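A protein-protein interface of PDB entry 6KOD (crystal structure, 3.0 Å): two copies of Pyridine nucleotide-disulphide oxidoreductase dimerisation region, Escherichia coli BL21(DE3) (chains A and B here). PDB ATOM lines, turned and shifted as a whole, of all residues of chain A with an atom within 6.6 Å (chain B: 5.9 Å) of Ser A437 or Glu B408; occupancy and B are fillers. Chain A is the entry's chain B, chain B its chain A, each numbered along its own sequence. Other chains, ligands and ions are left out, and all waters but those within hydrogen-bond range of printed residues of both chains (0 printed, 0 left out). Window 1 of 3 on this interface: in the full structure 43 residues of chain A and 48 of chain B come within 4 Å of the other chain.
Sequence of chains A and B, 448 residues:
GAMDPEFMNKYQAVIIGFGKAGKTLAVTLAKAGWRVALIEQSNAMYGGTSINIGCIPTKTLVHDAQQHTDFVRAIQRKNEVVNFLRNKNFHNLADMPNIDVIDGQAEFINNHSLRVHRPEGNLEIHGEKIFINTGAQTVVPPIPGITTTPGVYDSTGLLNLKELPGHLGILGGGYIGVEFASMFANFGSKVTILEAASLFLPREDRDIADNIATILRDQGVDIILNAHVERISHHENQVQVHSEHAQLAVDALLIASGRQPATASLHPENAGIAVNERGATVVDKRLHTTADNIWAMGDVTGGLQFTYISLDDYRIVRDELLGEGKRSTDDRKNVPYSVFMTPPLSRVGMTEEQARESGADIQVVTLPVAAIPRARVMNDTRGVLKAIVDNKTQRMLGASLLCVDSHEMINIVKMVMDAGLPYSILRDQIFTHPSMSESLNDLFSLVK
The side-chain hydroxyl of Thr A432 lies within hydrogen-bond range of the backbone carbonyl oxygen of His B407 (2.6 Å).
The side-chain carboxylate (OE1) of Glu B408 lies within hydrogen-bond range of the backbone NH (N) of Met A436, 2.9 Å away.
The side-chain amide nitrogen of Asn B411 is in hydrogen-bond range of the side-chain hydroxyl of Thr A432, at 3.1 Å.
ND2 of Asn B411 lies within hydrogen-bond range of OG of Ser A437 (3.0 Å).
The side-chain carboxylate of Glu B408 sits at hydrogen-bond distance from the side-chain hydroxyl of Ser A437, at 2.9 Å.
The side-chain carboxylate (OD1) of Asp A405 sits close to the side-chain carboxylate (OD1) of Asp B405 (3.3 Å).
N of Ser B437 sits at hydrogen-bond distance from OE2 of Glu A408.
The side-chain hydroxyl (OG) of Ser B346 sits at hydrogen-bond distance from the backbone NH (N) of His B407 (2.9 Å).
ND2 of Asn B411 lies within hydrogen-bond range of O of His B407 (3.0 Å).
N of Ser A435 is in hydrogen-bond range of OE2 of Glu A438, 3.0 Å away.
The side-chain carboxylate (OE1) of Glu B408 lies close to a ring nitrogen (NE2) of His B407 (3.4 Å).
The side-chain hydroxyl of Ser A435 sits at hydrogen-bond distance from the backbone NH of Ser A437 (3.2 Å).
NE of Arg A374 sits close to SD of Met A378 (3.6 Å).
NH1 of Arg A374 touches NE2 of His B407, 3.8 Å away.
Glu A408 touches Asp B405 (OE1 to OD2, 3.7 Å).
CD1 of Ile A412 touches CB of Asn B411, 3.9 Å away.
Ile A412 touches Ile B412 (CG1 to CG1, 3.6 Å).
Asn B411 touches Phe A431.
Thr A432 touches Ile B410.
OE1 of Glu B408 touches CB of Ser A435, at 3.4 Å.
Ser A437 touches just these residues of chain B: Glu B408 and Asn B411.
Printed residues of chain A within 4 Å of Glu B408: Ser A435 (3.4 Å), Met A436 (2.9 Å) and Ser A437 (2.9 Å).
Of the printed residues of chain B, Ile A412 touches Asn B411 and Ile B412.
Of the printed residues of chain B, Asp A405 touches Asp B405.
Printed residues of chain B within 4 Å of Phe A431: Asn B411 (3.6 Å).
Of the printed residues of chain B, Glu A408 touches Asp B405 (3.7 Å) and Ser B437 (2.4 Å).
Of the printed residues of chain A, Ile B412 touches Ile A412.
The nearest residue of chain B that does not touch Ser A437 is His B407 (4.8 Å).
Printed residues of chain A that touch a printed residue of chain B: Arg A374, Asp A405, Glu A408, Ile A412, Phe A431, Thr A432, Ser A435, Met A436 and Ser A437.
Along chain A the printed residues that touch a printed residue of chain B span positions 374 to 437.
Of the 10 printed residues of chain B, 7 touch a printed residue of chain A.
Printed residues of chain B that touch a printed residue of chain A: Asp B405, His B407, Glu B408, Ile B410, Asn B411, Ile B412 and Ser B437.
Along chain B the printed residues that touch a printed residue of chain A span positions 405 to 437.
Among the printed residues, 14 pairs touch across the chains.
Asp A405 touches its own counterpart, Asp B405.
Glu A408 touches Asp B405, but with the chains exchanged Asp A405 does not touch Glu B408 (4.4 Å).
Glu A408 touches Ser B437, and with the chains exchanged Ser A437 touches Glu B408.
Ile B412 touches its own counterpart, Ile A412.
5 positions are printed for both chains.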
ATOM      1  N   ARG A 374     -15.321  27.011  -4.847  1.00  0.00           N
ATOM      2  CA  ARG A 374     -14.853  25.825  -5.555  1.00  0.00           C
ATOM      3  C   ARG A 374     -14.018  24.930  -4.650  1.00  0.00           C
ATOM      4  O   ARG A 374     -14.070  23.701  -4.777  1.00  0.00           O
ATOM      5  CB  ARG A 374     -14.054  26.232  -6.792  1.00  0.00           C
ATOM      6  CG  ARG A 374     -13.338  25.086  -7.483  1.00  0.00           C
ATOM      7  CD  ARG A 374     -14.288  24.218  -8.286  1.00  0.00           C
ATOM      8  NE  ARG A 374     -13.704  22.910  -8.565  1.00  0.00           N
ATOM      9  CZ  ARG A 374     -14.111  22.098  -9.535  1.00  0.00           C
ATOM     10  NH1 ARG A 374     -13.518  20.924  -9.711  1.00  0.00           N
ATOM     11  NH2 ARG A 374     -15.111  22.457 -10.328  1.00  0.00           N
ATOM     12  N   MET A 378     -14.794  20.806  -3.950  1.00  0.00           N
ATOM     13  CA  MET A 378     -13.867  19.685  -4.001  1.00  0.00           C
ATOM     14  C   MET A 378     -13.635  19.040  -2.639  1.00  0.00           C
ATOM     15  O   MET A 378     -12.779  18.156  -2.525  1.00  0.00           O
ATOM     16  CB  MET A 378     -12.538  20.142  -4.604  1.00  0.00           C
ATOM     17  CG  MET A 378     -12.671  20.658  -6.028  1.00  0.00           C
ATOM     18  SD  MET A 378     -11.095  21.126  -6.761  1.00  0.00           S
ATOM     19  CE  MET A 378     -10.154  19.618  -6.537  1.00  0.00           C
ATOM     20  N   ASP A 405      -5.259  22.192  -6.330  1.00  0.00           N
ATOM     21  CA  ASP A 405      -4.992  22.604  -7.711  1.00  0.00           C
ATOM     22  C   ASP A 405      -4.139  23.870  -7.783  1.00  0.00           C
ATOM     23  O   ASP A 405      -4.246  24.650  -8.731  1.00  0.00           O
ATOM     24  CB  ASP A 405      -6.295  22.791  -8.498  1.00  0.00           C
ATOM     25  CG  ASP A 405      -6.854  21.480  -9.020  1.00  0.00           C
ATOM     26  OD1 ASP A 405      -7.908  21.506  -9.690  1.00  0.00           O
ATOM     27  OD2 ASP A 405      -6.240  20.424  -8.762  1.00  0.00           O
ATOM     28  N   GLU A 408      -1.671  24.498 -10.951  1.00  0.00           N
ATOM     29  CA  GLU A 408      -2.120  25.110 -12.195  1.00  0.00           C
ATOM     30  C   GLU A 408      -2.388  26.602 -12.061  1.00  0.00           C
ATOM     31  O   GLU A 408      -2.154  27.352 -13.014  1.00  0.00           O
ATOM     32  CB  GLU A 408      -3.388  24.417 -12.707  1.00  0.00           C
ATOM     33  CG  GLU A 408      -3.436  22.924 -12.436  1.00  0.00           C
ATOM     34  CD  GLU A 408      -2.908  22.100 -13.593  1.00  0.00           C
ATOM     35  OE1 GLU A 408      -3.222  20.893 -13.649  1.00  0.00           O
ATOM     36  OE2 GLU A 408      -2.180  22.655 -14.443  1.00  0.00           O
ATOM     37  N   MET A 409      -2.876  27.048 -10.901  1.00  0.00           N
ATOM     38  CA  MET A 409      -3.035  28.479 -10.670  1.00  0.00           C
ATOM     39  C   MET A 409      -1.691  29.189 -10.634  1.00  0.00           C
ATOM     40  O   MET A 409      -1.604  30.366 -10.999  1.00  0.00           O
ATOM     41  CB  MET A 409      -3.779  28.728  -9.360  1.00  0.00           C
ATOM     42  CG  MET A 409      -5.036  27.901  -9.170  1.00  0.00           C
ATOM     43  SD  MET A 409      -5.694  28.101  -7.505  1.00  0.00           S
ATOM     44  CE  MET A 409      -5.248  29.804  -7.167  1.00  0.00           C
ATOM     45  N   ILE A 412      -0.586  30.869 -13.798  1.00  0.00           N
ATOM     46  CA  ILE A 412      -1.276  32.086 -14.215  1.00  0.00           C
ATOM     47  C   ILE A 412      -0.602  33.313 -13.615  1.00  0.00           C
ATOM     48  O   ILE A 412      -0.312  34.287 -14.320  1.00  0.00           O
ATOM     49  CB  ILE A 412      -2.767  32.019 -13.832  1.00  0.00           C
ATOM     50  CG1 ILE A 412      -3.368  30.676 -14.244  1.00  0.00           C
ATOM     51  CG2 ILE A 412      -3.534  33.162 -14.476  1.00  0.00           C
ATOM     52  CD1 ILE A 412      -4.876  30.638 -14.155  1.00  0.00           C
ATOM     53  N   LEU A 426      -4.925  40.358 -12.854  1.00  0.00           N
ATOM     54  CA  LEU A 426      -5.514  39.167 -12.253  1.00  0.00           C
ATOM     55  C   LEU A 426      -6.789  39.481 -11.483  1.00  0.00           C
ATOM     56  O   LEU A 426      -7.652  38.607 -11.342  1.00  0.00           O
ATOM     57  CB  LEU A 426      -4.499  38.487 -11.335  1.00  0.00           C
ATOM     58  CG  LEU A 426      -3.380  37.733 -12.053  1.00  0.00           C
ATOM     59  CD1 LEU A 426      -2.399  37.153 -11.044  1.00  0.00           C
ATOM     60  CD2 LEU A 426      -3.957  36.646 -12.953  1.00  0.00           C
ATOM     61  N   PHE A 431     -12.560  34.727 -15.439  1.00  0.00           N
ATOM     62  CA  PHE A 431     -12.117  33.353 -15.280  1.00  0.00           C
ATOM     63  C   PHE A 431     -13.291  32.398 -15.491  1.00  0.00           C
ATOM     64  O   PHE A 431     -14.409  32.804 -15.817  1.00  0.00           O
ATOM     65  CB  PHE A 431     -11.491  33.155 -13.899  1.00  0.00           C
ATOM     66  CG  PHE A 431     -10.121  33.753 -13.757  1.00  0.00           C
ATOM     67  CD1 PHE A 431      -9.042  33.222 -14.445  1.00  0.00           C
ATOM     68  CD2 PHE A 431      -9.909  34.841 -12.925  1.00  0.00           C
ATOM     69  CE1 PHE A 431      -7.779  33.766 -14.311  1.00  0.00           C
ATOM     70  CE2 PHE A 431      -8.647  35.389 -12.786  1.00  0.00           C
ATOM     71  CZ  PHE A 431      -7.581  34.849 -13.480  1.00  0.00           C
ATOM     72  N   THR A 432     -13.031  31.109 -15.299  1.00  0.00           N
ATOM     73  CA  THR A 432     -14.063  30.090 -15.409  1.00  0.00           C
ATOM     74  C   THR A 432     -14.750  29.884 -14.062  1.00  0.00           C
ATOM     75  O   THR A 432     -14.230  30.257 -13.008  1.00  0.00           O
ATOM     76  CB  THR A 432     -13.472  28.771 -15.910  1.00  0.00           C
ATOM     77  OG1 THR A 432     -12.159  28.592 -15.362  1.00  0.00           O
ATOM     78  CG2 THR A 432     -13.385  28.769 -17.431  1.00  0.00           C
ATOM     79  N   PRO A 434     -17.540  26.981 -11.962  1.00  0.00           N
ATOM     80  CA  PRO A 434     -16.716  27.195 -10.769  1.00  0.00           C
ATOM     81  C   PRO A 434     -15.294  26.690 -10.972  1.00  0.00           C
ATOM     82  O   PRO A 434     -15.098  25.603 -11.515  1.00  0.00           O
ATOM     83  CB  PRO A 434     -17.432  26.376  -9.683  1.00  0.00           C
ATOM     84  CG  PRO A 434     -18.575  25.659 -10.377  1.00  0.00           C
ATOM     85  CD  PRO A 434     -18.338  25.752 -11.848  1.00  0.00           C
ATOM     86  N   SER A 435     -14.312  27.477 -10.542  1.00  0.00           N
ATOM     87  CA  SER A 435     -12.917  27.110 -10.709  1.00  0.00           C
ATOM     88  C   SER A 435     -12.118  27.679  -9.545  1.00  0.00           C
ATOM     89  O   SER A 435     -12.660  28.335  -8.652  1.00  0.00           O
ATOM     90  CB  SER A 435     -12.370  27.612 -12.048  1.00  0.00           C
ATOM     91  OG  SER A 435     -11.893  28.942 -11.933  1.00  0.00           O
ATOM     92  N   MET A 436     -10.815  27.411  -9.560  1.00  0.00           N
ATOM     93  CA  MET A 436      -9.896  27.999  -8.603  1.00  0.00           C
ATOM     94  C   MET A 436      -8.980  29.033  -9.231  1.00  0.00           C
ATOM     95  O   MET A 436      -8.242  29.706  -8.505  1.00  0.00           O
ATOM     96  CB  MET A 436      -9.061  26.904  -7.930  1.00  0.00           C
ATOM     97  CG  MET A 436      -9.916  25.809  -7.348  1.00  0.00           C
ATOM     98  SD  MET A 436      -9.334  25.248  -5.751  1.00  0.00           S
ATOM     99  CE  MET A 436      -9.477  26.738  -4.778  1.00  0.00           C
ATOM    100  N   SER A 437      -8.997  29.171 -10.555  1.00  0.00           N
ATOM    101  CA  SER A 437      -8.347  30.319 -11.173  1.00  0.00           C
ATOM    102  C   SER A 437      -9.062  31.607 -10.788  1.00  0.00           C
ATOM    103  O   SER A 437      -8.417  32.628 -10.523  1.00  0.00           O
ATOM    104  CB  SER A 437      -8.313  30.149 -12.689  1.00  0.00           C
ATOM    105  OG  SER A 437      -7.474  29.069 -13.061  1.00  0.00           O
ATOM    106  N   GLU A 438     -10.395  31.569 -10.738  1.00  0.00           N
ATOM    107  CA  GLU A 438     -11.183  32.712 -10.295  1.00  0.00           C
ATOM    108  C   GLU A 438     -10.943  33.054  -8.834  1.00  0.00           C
ATOM    109  O   GLU A 438     -11.373  34.123  -8.385  1.00  0.00           O
ATOM    110  CB  GLU A 438     -12.670  32.441 -10.520  1.00  0.00           C
ATOM    111  CG  GLU A 438     -13.157  31.181  -9.839  1.00  0.00           C
ATOM    112  CD  GLU A 438     -14.648  31.182  -9.605  1.00  0.00           C
ATOM    113  OE1 GLU A 438     -15.259  32.270  -9.673  1.00  0.00           O
ATOM    114  OE2 GLU A 438     -15.207  30.094  -9.350  1.00  0.00           O
ATOM    115  N   SER A 439     -10.284  32.173  -8.079  1.00  0.00           N
ATOM    116  CA  SER A 439      -9.869  32.529  -6.729  1.00  0.00           C
ATOM    117  C   SER A 439      -8.967  33.758  -6.733  1.00  0.00           C
ATOM    118  O   SER A 439      -8.940  34.512  -5.753  1.00  0.00           O
ATOM    119  CB  SER A 439      -9.166  31.338  -6.074  1.00  0.00           C
ATOM    120  OG  SER A 439      -8.317  31.756  -5.026  1.00  0.00           O
ATOM    121  N   LEU A 440      -8.236  33.985  -7.828  1.00  0.00           N
ATOM    122  CA  LEU A 440      -7.396  35.171  -7.938  1.00  0.00           C
ATOM    123  C   LEU A 440      -8.211  36.441  -8.144  1.00  0.00           C
ATOM    124  O   LEU A 440      -7.692  37.536  -7.905  1.00  0.00           O
ATOM    125  CB  LEU A 440      -6.395  35.004  -9.084  1.00  0.00           C
ATOM    126  CG  LEU A 440      -5.325  33.934  -8.867  1.00  0.00           C
ATOM    127  CD1 LEU A 440      -4.469  33.746 -10.115  1.00  0.00           C
ATOM    128  CD2 LEU A 440      -4.463  34.287  -7.664  1.00  0.00           C
ATOM    129  N   ASN A 441      -9.465  36.321  -8.589  1.00  0.00           N
ATOM    130  CA  ASN A 441     -10.329  37.495  -8.684  1.00  0.00           C
ATOM    131  C   ASN A 441     -10.571  38.103  -7.309  1.00  0.00           C
ATOM    132  O   ASN A 441     -10.491  39.326  -7.138  1.00  0.00           O
ATOM    133  CB  ASN A 441     -11.659  37.121  -9.339  1.00  0.00           C
ATOM    134  CG  ASN A 441     -11.670  37.373 -10.832  1.00  0.00           C
ATOM    135  OD1 ASN A 441     -10.677  37.817 -11.407  1.00  0.00           O
ATOM    136  ND2 ASN A 441     -12.801  37.092 -11.469  1.00  0.00           N
ATOM    137  N   SER B 346     -13.295  22.506 -21.862  1.00  0.00           N
ATOM    138  CA  SER B 346     -13.194  23.952 -21.748  1.00  0.00           C
ATOM    139  C   SER B 346     -12.770  24.512 -23.094  1.00  0.00           C
ATOM    140  O   SER B 346     -11.922  23.928 -23.777  1.00  0.00           O
ATOM    141  CB  SER B 346     -12.181  24.341 -20.673  1.00  0.00           C
ATOM    142  OG  SER B 346     -12.459  23.665 -19.459  1.00  0.00           O
ATOM    143  N   ASP B 405      -9.043  18.850 -15.475  1.00  0.00           N
ATOM    144  CA  ASP B 405      -8.556  20.174 -15.086  1.00  0.00           C
ATOM    145  C   ASP B 405      -8.485  21.142 -16.264  1.00  0.00           C
ATOM    146  O   ASP B 405      -7.744  22.129 -16.213  1.00  0.00           O
ATOM    147  CB  ASP B 405      -7.189  20.086 -14.395  1.00  0.00           C
ATOM    148  CG  ASP B 405      -7.288  19.579 -12.973  1.00  0.00           C
ATOM    149  OD1 ASP B 405      -8.396  19.634 -12.399  1.00  0.00           O
ATOM    150  OD2 ASP B 405      -6.258  19.127 -12.430  1.00  0.00           O
ATOM    151  N   SER B 406      -9.249  20.885 -17.328  1.00  0.00           N
ATOM    152  CA  SER B 406      -9.263  21.802 -18.463  1.00  0.00           C
ATOM    153  C   SER B 406      -9.867  23.150 -18.089  1.00  0.00           C
ATOM    154  O   SER B 406      -9.523  24.171 -18.694  1.00  0.00           O
ATOM    155  CB  SER B 406     -10.028  21.183 -19.634  1.00  0.00           C
ATOM    156  OG  SER B 406     -11.420  21.140 -19.374  1.00  0.00           O
ATOM    157  N   HIS B 407     -10.764  23.176 -17.101  1.00  0.00           N
ATOM    158  CA  HIS B 407     -11.340  24.430 -16.630  1.00  0.00           C
ATOM    159  C   HIS B 407     -10.313  25.336 -15.963  1.00  0.00           C
ATOM    160  O   HIS B 407     -10.643  26.483 -15.640  1.00  0.00           O
ATOM    161  CB  HIS B 407     -12.488  24.146 -15.661  1.00  0.00           C
ATOM    162  CG  HIS B 407     -12.075  23.365 -14.453  1.00  0.00           C
ATOM    163  ND1 HIS B 407     -11.757  22.026 -14.507  1.00  0.00           N
ATOM    164  CD2 HIS B 407     -11.924  23.737 -13.161  1.00  0.00           C
ATOM    165  CE1 HIS B 407     -11.428  21.605 -13.299  1.00  0.00           C
ATOM    166  NE2 HIS B 407     -11.520  22.624 -12.464  1.00  0.00           N
ATOM    167  N   GLU B 408      -9.090  24.853 -15.746  1.00  0.00           N
ATOM    168  CA  GLU B 408      -8.014  25.667 -15.198  1.00  0.00           C
ATOM    169  C   GLU B 408      -6.930  26.007 -16.209  1.00  0.00           C
ATOM    170  O   GLU B 408      -6.270  27.037 -16.061  1.00  0.00           O
ATOM    171  CB  GLU B 408      -7.372  24.961 -13.997  1.00  0.00           C
ATOM    172  CG  GLU B 408      -8.373  24.449 -12.976  1.00  0.00           C
ATOM    173  CD  GLU B 408      -8.796  25.515 -11.982  1.00  0.00           C
ATOM    174  OE1 GLU B 408      -9.881  25.374 -11.385  1.00  0.00           O
ATOM    175  OE2 GLU B 408      -8.046  26.495 -11.796  1.00  0.00           O
ATOM    176  N   MET B 409      -6.728  25.171 -17.233  1.00  0.00           N
ATOM    177  CA  MET B 409      -5.748  25.496 -18.263  1.00  0.00           C
ATOM    178  C   MET B 409      -6.255  26.568 -19.217  1.00  0.00           C
ATOM    179  O   MET B 409      -5.458  27.363 -19.727  1.00  0.00           O
ATOM    180  CB  MET B 409      -5.371  24.250 -19.068  1.00  0.00           C
ATOM    181  CG  MET B 409      -5.344  22.952 -18.290  1.00  0.00           C
ATOM    182  SD  MET B 409      -5.359  21.531 -19.406  1.00  0.00           S
ATOM    183  CE  MET B 409      -4.218  22.081 -20.673  1.00  0.00           C
ATOM    184  N   ILE B 410      -7.566  26.600 -19.473  1.00  0.00           N
ATOM    185  CA  ILE B 410      -8.111  27.509 -20.472  1.00  0.00           C
ATOM    186  C   ILE B 410      -7.936  28.969 -20.067  1.00  0.00           C
ATOM    187  O   ILE B 410      -7.884  29.848 -20.935  1.00  0.00           O
ATOM    188  CB  ILE B 410      -9.592  27.172 -20.740  1.00  0.00           C
ATOM    189  CG1 ILE B 410     -10.020  27.695 -22.112  1.00  0.00           C
ATOM    190  CG2 ILE B 410     -10.488  27.719 -19.637  1.00  0.00           C
ATOM    191  CD1 ILE B 410      -9.579  26.815 -23.259  1.00  0.00           C
ATOM    192  N   ASN B 411      -7.824  29.249 -18.766  1.00  0.00           N
ATOM    193  CA  ASN B 411      -7.579  30.617 -18.325  1.00  0.00           C
ATOM    194  C   ASN B 411      -6.182  31.087 -18.709  1.00  0.00           C
ATOM    195  O   ASN B 411      -5.980  32.278 -18.969  1.00  0.00           O
ATOM    196  CB  ASN B 411      -7.791  30.721 -16.815  1.00  0.00           C
ATOM    197  CG  ASN B 411      -9.119  30.134 -16.374  1.00  0.00           C
ATOM    198  OD1 ASN B 411     -10.184  30.658 -16.704  1.00  0.00           O
ATOM    199  ND2 ASN B 411      -9.063  29.031 -15.638  1.00  0.00           N
ATOM    200  N   ILE B 412      -5.209  30.174 -18.750  1.00  0.00           N
ATOM    201  CA  ILE B 412      -3.886  30.530 -19.252  1.00  0.00           C
ATOM    202  C   ILE B 412      -3.948  30.800 -20.748  1.00  0.00           C
ATOM    203  O   ILE B 412      -3.293  31.717 -21.258  1.00  0.00           O
ATOM    204  CB  ILE B 412      -2.867  29.425 -18.919  1.00  0.00           C
ATOM    205  CG1 ILE B 412      -2.941  29.059 -17.433  1.00  0.00           C
ATOM    206  CG2 ILE B 412      -1.459  29.864 -19.290  1.00  0.00           C
ATOM    207  CD1 ILE B 412      -1.885  28.065 -16.987  1.00  0.00           C
ATOM    208  N   SER B 437      -1.356  22.015 -17.094  1.00  0.00           N
ATOM    209  CA  SER B 437      -1.031  23.221 -17.850  1.00  0.00           C
ATOM    210  C   SER B 437       0.216  23.033 -18.704  1.00  0.00           C
ATOM    211  O   SER B 437       0.360  23.688 -19.745  1.00  0.00           O
ATOM    212  CB  SER B 437      -0.838  24.402 -16.898  1.00  0.00           C
ATOM    213  OG  SER B 437      -1.888  24.478 -15.951  1.00  0.00           O
